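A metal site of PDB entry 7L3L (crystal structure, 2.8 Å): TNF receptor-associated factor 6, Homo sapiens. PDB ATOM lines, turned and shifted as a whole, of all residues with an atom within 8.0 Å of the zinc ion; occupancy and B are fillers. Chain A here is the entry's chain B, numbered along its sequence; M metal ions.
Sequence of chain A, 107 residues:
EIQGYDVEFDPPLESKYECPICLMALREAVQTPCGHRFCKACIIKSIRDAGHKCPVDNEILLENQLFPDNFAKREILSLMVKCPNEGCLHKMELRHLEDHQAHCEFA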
ATOM      1  N   ILE A   2     -19.975  16.560  24.381  1.00  0.00           N
ATOM      2  CA  ILE A   2     -18.572  16.167  24.498  1.00  0.00           C
ATOM      3  C   ILE A   2     -17.980  16.927  25.673  1.00  0.00           C
ATOM      4  O   ILE A   2     -17.999  18.170  25.695  1.00  0.00           O
ATOM      5  CB  ILE A   2     -17.798  16.469  23.205  1.00  0.00           C
ATOM      6  CG1 ILE A   2     -18.659  16.150  21.981  1.00  0.00           C
ATOM      7  CG2 ILE A   2     -16.497  15.695  23.167  1.00  0.00           C
ATOM      8  CD1 ILE A   2     -19.280  17.363  21.311  1.00  0.00           C
ATOM      9  N   GLN A   3     -17.480  16.197  26.679  1.00  0.00           N
ATOM     10  CA  GLN A   3     -17.011  16.827  27.899  1.00  0.00           C
ATOM     11  C   GLN A   3     -15.518  16.613  28.154  1.00  0.00           C
ATOM     12  O   GLN A   3     -14.781  17.604  28.232  1.00  0.00           O
ATOM     13  CB  GLN A   3     -17.841  16.306  29.077  1.00  0.00           C
ATOM     14  CG  GLN A   3     -19.305  16.628  28.931  1.00  0.00           C
ATOM     15  CD  GLN A   3     -20.160  15.800  29.868  1.00  0.00           C
ATOM     16  OE1 GLN A   3     -20.186  16.039  31.078  1.00  0.00           O
ATOM     17  NE2 GLN A   3     -20.857  14.819  29.312  1.00  0.00           N
ATOM     18  N   GLY A   4     -15.046  15.385  28.264  1.00  0.00           N
ATOM     19  CA  GLY A   4     -13.676  15.166  28.659  1.00  0.00           C
ATOM     20  C   GLY A   4     -13.301  13.698  28.525  1.00  0.00           C
ATOM     21  O   GLY A   4     -14.026  12.908  27.932  1.00  0.00           O
ATOM     22  N   TYR A   5     -12.153  13.351  29.101  1.00  0.00           N
ATOM     23  CA  TYR A   5     -11.654  11.971  29.044  1.00  0.00           C
ATOM     24  C   TYR A   5     -12.133  11.182  30.256  1.00  0.00           C
ATOM     25  O   TYR A   5     -11.891  11.583  31.412  1.00  0.00           O
ATOM     26  CB  TYR A   5     -10.127  11.960  28.961  1.00  0.00           C
ATOM     27  CG  TYR A   5      -9.552  12.479  27.659  1.00  0.00           C
ATOM     28  CD1 TYR A   5      -9.761  11.792  26.459  1.00  0.00           C
ATOM     29  CD2 TYR A   5      -8.803  13.644  27.624  1.00  0.00           C
ATOM     30  CE1 TYR A   5      -9.238  12.258  25.266  1.00  0.00           C
ATOM     31  CE2 TYR A   5      -8.275  14.117  26.437  1.00  0.00           C
ATOM     32  CZ  TYR A   5      -8.496  13.414  25.262  1.00  0.00           C
ATOM     33  OH  TYR A   5      -7.977  13.891  24.077  1.00  0.00           O
ATOM     34  N   GLU A  18      -7.361  19.102  35.068  1.00  0.00           N
ATOM     35  CA  GLU A  18      -8.755  18.737  35.214  1.00  0.00           C
ATOM     36  C   GLU A  18      -9.636  19.908  34.822  1.00  0.00           C
ATOM     37  O   GLU A  18      -9.395  21.038  35.267  1.00  0.00           O
ATOM     38  CB  GLU A  18      -9.057  18.299  36.657  1.00  0.00           C
ATOM     39  CG  GLU A  18     -10.522  18.071  36.952  1.00  0.00           C
ATOM     40  CD  GLU A  18     -10.751  17.482  38.326  1.00  0.00           C
ATOM     41  OE1 GLU A  18     -10.176  16.408  38.621  1.00  0.00           O
ATOM     42  OE2 GLU A  18     -11.487  18.102  39.132  1.00  0.00           O
ATOM     43  N   CYS A  19     -10.641  19.643  33.999  1.00  0.00           N
ATOM     44  CA  CYS A  19     -11.532  20.704  33.537  1.00  0.00           C
ATOM     45  C   CYS A  19     -12.494  21.110  34.650  1.00  0.00           C
ATOM     46  O   CYS A  19     -13.222  20.256  35.167  1.00  0.00           O
ATOM     47  CB  CYS A  19     -12.320  20.241  32.317  1.00  0.00           C
ATOM     48  SG  CYS A  19     -13.641  21.363  31.818  1.00  0.00           S
ATOM     49  N   PRO A  20     -12.530  22.377  35.048  1.00  0.00           N
ATOM     50  CA  PRO A  20     -13.455  22.801  36.101  1.00  0.00           C
ATOM     51  C   PRO A  20     -14.924  22.678  35.717  1.00  0.00           C
ATOM     52  O   PRO A  20     -15.774  22.778  36.605  1.00  0.00           O
ATOM     53  CB  PRO A  20     -13.063  24.257  36.368  1.00  0.00           C
ATOM     54  CG  PRO A  20     -11.679  24.392  35.824  1.00  0.00           C
ATOM     55  CD  PRO A  20     -11.614  23.468  34.650  1.00  0.00           C
ATOM     56  N   ILE A  21     -15.249  22.497  34.436  1.00  0.00           N
ATOM     57  CA  ILE A  21     -16.654  22.377  34.037  1.00  0.00           C
ATOM     58  C   ILE A  21     -17.095  20.926  34.140  1.00  0.00           C
ATOM     59  O   ILE A  21     -17.958  20.588  34.967  1.00  0.00           O
ATOM     60  CB  ILE A  21     -16.883  22.916  32.619  1.00  0.00           C
ATOM     61  CG1 ILE A  21     -16.817  24.434  32.597  1.00  0.00           C
ATOM     62  CG2 ILE A  21     -18.229  22.443  32.081  1.00  0.00           C
ATOM     63  CD1 ILE A  21     -17.155  25.040  31.251  1.00  0.00           C
ATOM     64  N   CYS A  22     -16.503  20.050  33.334  1.00  0.00           N
ATOM     65  CA  CYS A  22     -16.941  18.663  33.254  1.00  0.00           C
ATOM     66  C   CYS A  22     -16.224  17.767  34.249  1.00  0.00           C
ATOM     67  O   CYS A  22     -16.542  16.570  34.320  1.00  0.00           O
ATOM     68  CB  CYS A  22     -16.721  18.140  31.835  1.00  0.00           C
ATOM     69  SG  CYS A  22     -15.003  18.015  31.331  1.00  0.00           S
ATOM     70  N   LEU A  23     -15.273  18.301  35.019  1.00  0.00           N
ATOM     71  CA  LEU A  23     -14.556  17.546  36.042  1.00  0.00           C
ATOM     72  C   LEU A  23     -13.847  16.324  35.442  1.00  0.00           C
ATOM     73  O   LEU A  23     -13.868  15.236  36.013  1.00  0.00           O
ATOM     74  CB  LEU A  23     -15.485  17.130  37.179  1.00  0.00           C
ATOM     75  CG  LEU A  23     -16.083  18.277  37.992  1.00  0.00           C
ATOM     76  CD1 LEU A  23     -16.847  17.746  39.181  1.00  0.00           C
ATOM     77  CD2 LEU A  23     -14.979  19.228  38.436  1.00  0.00           C
ATOM     78  N   MET A  24     -13.220  16.515  34.289  1.00  0.00           N
ATOM     79  CA  MET A  24     -12.507  15.452  33.614  1.00  0.00           C
ATOM     80  C   MET A  24     -11.274  16.023  32.925  1.00  0.00           C
ATOM     81  O   MET A  24     -11.109  17.248  32.820  1.00  0.00           O
ATOM     82  CB  MET A  24     -13.419  14.725  32.616  1.00  0.00           C
ATOM     83  CG  MET A  24     -14.113  13.513  33.214  1.00  0.00           C
ATOM     84  SD  MET A  24     -15.731  13.162  32.497  1.00  0.00           S
ATOM     85  CE  MET A  24     -15.286  12.447  30.926  1.00  0.00           C
ATOM     86  N   ALA A  25     -10.394  15.131  32.485  1.00  0.00           N
ATOM     87  CA  ALA A  25      -9.154  15.559  31.845  1.00  0.00           C
ATOM     88  C   ALA A  25      -9.458  16.335  30.570  1.00  0.00           C
ATOM     89  O   ALA A  25     -10.309  15.925  29.760  1.00  0.00           O
ATOM     90  CB  ALA A  25      -8.263  14.362  31.527  1.00  0.00           C
ATOM     91  N   LEU A  26      -8.755  17.450  30.394  1.00  0.00           N
ATOM     92  CA  LEU A  26      -9.097  18.395  29.339  1.00  0.00           C
ATOM     93  C   LEU A  26      -9.008  17.747  27.969  1.00  0.00           C
ATOM     94  O   LEU A  26      -8.033  17.059  27.649  1.00  0.00           O
ATOM     95  CB  LEU A  26      -8.147  19.599  29.414  1.00  0.00           C
ATOM     96  CG  LEU A  26      -7.984  20.237  30.779  1.00  0.00           C
ATOM     97  CD1 LEU A  26      -6.638  20.910  30.892  1.00  0.00           C
ATOM     98  CD2 LEU A  26      -9.081  21.240  31.012  1.00  0.00           C
ATOM     99  N   ARG A  27     -10.038  17.967  27.151  1.00  0.00           N
ATOM    100  CA  ARG A  27     -10.080  17.479  25.784  1.00  0.00           C
ATOM    101  C   ARG A  27      -9.925  18.657  24.843  1.00  0.00           C
ATOM    102  O   ARG A  27     -10.776  19.566  24.838  1.00  0.00           O
ATOM    103  CB  ARG A  27     -11.388  16.729  25.515  1.00  0.00           C
ATOM    104  CG  ARG A  27     -11.694  16.573  24.046  1.00  0.00           C
ATOM    105  CD  ARG A  27     -12.883  15.674  23.835  1.00  0.00           C
ATOM    106  NE  ARG A  27     -12.460  14.278  23.768  1.00  0.00           N
ATOM    107  CZ  ARG A  27     -12.887  13.343  24.596  1.00  0.00           C
ATOM    108  NH1 ARG A  27     -13.753  13.649  25.553  1.00  0.00           N
ATOM    109  NH2 ARG A  27     -12.466  12.087  24.463  1.00  0.00           N
ATOM    110  N   ARG A  37      -7.703  26.606  32.590  1.00  0.00           N
ATOM    111  CA  ARG A  37      -7.823  25.685  31.478  1.00  0.00           C
ATOM    112  C   ARG A  37      -9.191  25.020  31.486  1.00  0.00           C
ATOM    113  O   ARG A  37      -9.729  24.682  32.537  1.00  0.00           O
ATOM    114  CB  ARG A  37      -6.725  24.607  31.551  1.00  0.00           C
ATOM    115  CG  ARG A  37      -5.316  25.167  31.708  1.00  0.00           C
ATOM    116  CD  ARG A  37      -4.266  24.060  31.684  1.00  0.00           C
ATOM    117  NE  ARG A  37      -2.908  24.582  31.657  1.00  0.00           N
ATOM    118  CZ  ARG A  37      -2.072  24.586  32.699  1.00  0.00           C
ATOM    119  NH1 ARG A  37      -2.474  24.083  33.861  1.00  0.00           N
ATOM    120  NH2 ARG A  37      -0.857  25.094  32.576  1.00  0.00           N
ATOM    121  N   PHE A  38      -9.759  24.846  30.289  1.00  0.00           N
ATOM    122  CA  PHE A  38     -11.026  24.141  30.104  1.00  0.00           C
ATOM    123  C   PHE A  38     -10.892  23.259  28.869  1.00  0.00           C
ATOM    124  O   PHE A  38      -9.933  23.366  28.106  1.00  0.00           O
ATOM    125  CB  PHE A  38     -12.212  25.099  29.930  1.00  0.00           C
ATOM    126  CG  PHE A  38     -12.397  26.076  31.068  1.00  0.00           C
ATOM    127  CD1 PHE A  38     -11.717  27.282  31.088  1.00  0.00           C
ATOM    128  CD2 PHE A  38     -13.294  25.803  32.094  1.00  0.00           C
ATOM    129  CE1 PHE A  38     -11.903  28.187  32.124  1.00  0.00           C
ATOM    130  CE2 PHE A  38     -13.480  26.702  33.138  1.00  0.00           C
ATOM    131  CZ  PHE A  38     -12.787  27.894  33.147  1.00  0.00           C
ATOM    132  N   CYS A  39     -11.874  22.392  28.670  1.00  0.00           N
ATOM    133  CA  CYS A  39     -12.018  21.760  27.366  1.00  0.00           C
ATOM    134  C   CYS A  39     -12.587  22.782  26.392  1.00  0.00           C
ATOM    135  O   CYS A  39     -13.322  23.685  26.766  1.00  0.00           O
ATOM    136  CB  CYS A  39     -12.940  20.548  27.460  1.00  0.00           C
ATOM    137  SG  CYS A  39     -12.694  19.549  28.933  1.00  0.00           S
ATOM    138  N   LYS A  40     -12.214  22.634  25.115  1.00  0.00           N
ATOM    139  CA  LYS A  40     -12.718  23.565  24.109  1.00  0.00           C
ATOM    140  C   LYS A  40     -14.241  23.503  24.024  1.00  0.00           C
ATOM    141  O   LYS A  40     -14.907  24.539  23.964  1.00  0.00           O
ATOM    142  CB  LYS A  40     -12.104  23.273  22.749  1.00  0.00           C
ATOM    143  CG  LYS A  40     -12.531  24.272  21.665  1.00  0.00           C
ATOM    144  CD  LYS A  40     -11.670  24.152  20.417  1.00  0.00           C
ATOM    145  CE  LYS A  40     -11.707  22.736  19.854  1.00  0.00           C
ATOM    146  NZ  LYS A  40     -10.595  22.484  18.892  1.00  0.00           N
ATOM    147  N   ALA A  41     -14.803  22.291  24.040  1.00  0.00           N
ATOM    148  CA  ALA A  41     -16.253  22.152  23.936  1.00  0.00           C
ATOM    149  C   ALA A  41     -16.953  22.697  25.186  1.00  0.00           C
ATOM    150  O   ALA A  41     -17.960  23.406  25.083  1.00  0.00           O
ATOM    151  CB  ALA A  41     -16.625  20.692  23.708  1.00  0.00           C
ATOM    152  N   CYS A  42     -16.436  22.370  26.369  1.00  0.00           N
ATOM    153  CA  CYS A  42     -17.103  22.763  27.611  1.00  0.00           C
ATOM    154  C   CYS A  42     -17.187  24.282  27.744  1.00  0.00           C
ATOM    155  O   CYS A  42     -18.236  24.827  28.105  1.00  0.00           O
ATOM    156  CB  CYS A  42     -16.386  22.158  28.816  1.00  0.00           C
ATOM    157  SG  CYS A  42     -16.443  20.349  28.881  1.00  0.00           S
ATOM    158  N   ILE A  43     -16.089  24.980  27.454  1.00  0.00           N
ATOM    159  CA  ILE A  43     -16.038  26.401  27.757  1.00  0.00           C
ATOM    160  C   ILE A  43     -16.877  27.193  26.764  1.00  0.00           C
ATOM    161  O   ILE A  43     -17.546  28.170  27.143  1.00  0.00           O
ATOM    162  CB  ILE A  43     -14.574  26.896  27.797  1.00  0.00           C
ATOM    163  CG1 ILE A  43     -14.524  28.385  28.159  1.00  0.00           C
ATOM    164  CG2 ILE A  43     -13.876  26.650  26.474  1.00  0.00           C
ATOM    165  CD1 ILE A  43     -15.257  28.739  29.425  1.00  0.00           C
HETATM  166 ZN    ZN M   1     -14.569  19.922  30.163  1.00  0.00          ZN
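The side-chain sulfur of Cys 22 lies close to the backbone carbonyl oxygen of Gln 3.
SG of Cys 19 lies close to N of Ile 21, 3.3 Å away.
The side-chain sulfur (SG) of Cys 42 sits close to the backbone carbonyl oxygen (O) of Gln 3 (3.3 Å).
The backbone NH (N) of Cys 19 is in hydrogen-bond range of the backbone carbonyl oxygen (O) of Met 24 (2.7 Å).
O of Gln 3 lies close to SG of Cys 39 (2.9 Å).
The side-chain sulfur of Cys 39 lies close to the backbone NH of Arg 27.
The side-chain sulfur (SG) of Cys 22 sits close to the backbone NH (N) of Met 24, at 3.8 Å.
Residues that only touch the zinc ion: Gln 3.
Of the 21 residues printed, 5 come within 4 Å of the zinc ion.
The nearest printed residue that does not touch the zinc ion is Ile 21 (4.5 Å).
The side-chain sulfur (SG) of Cys 39 is bound to the zinc ion, at 2.3 Å.
The zinc ion is bound by SG of Cys 22 (2.3 Å).
SG of Cys 42 binds the zinc ion, 2.3 Å away.
SG of Cys 19 binds the zinc ion (2.4 Å).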
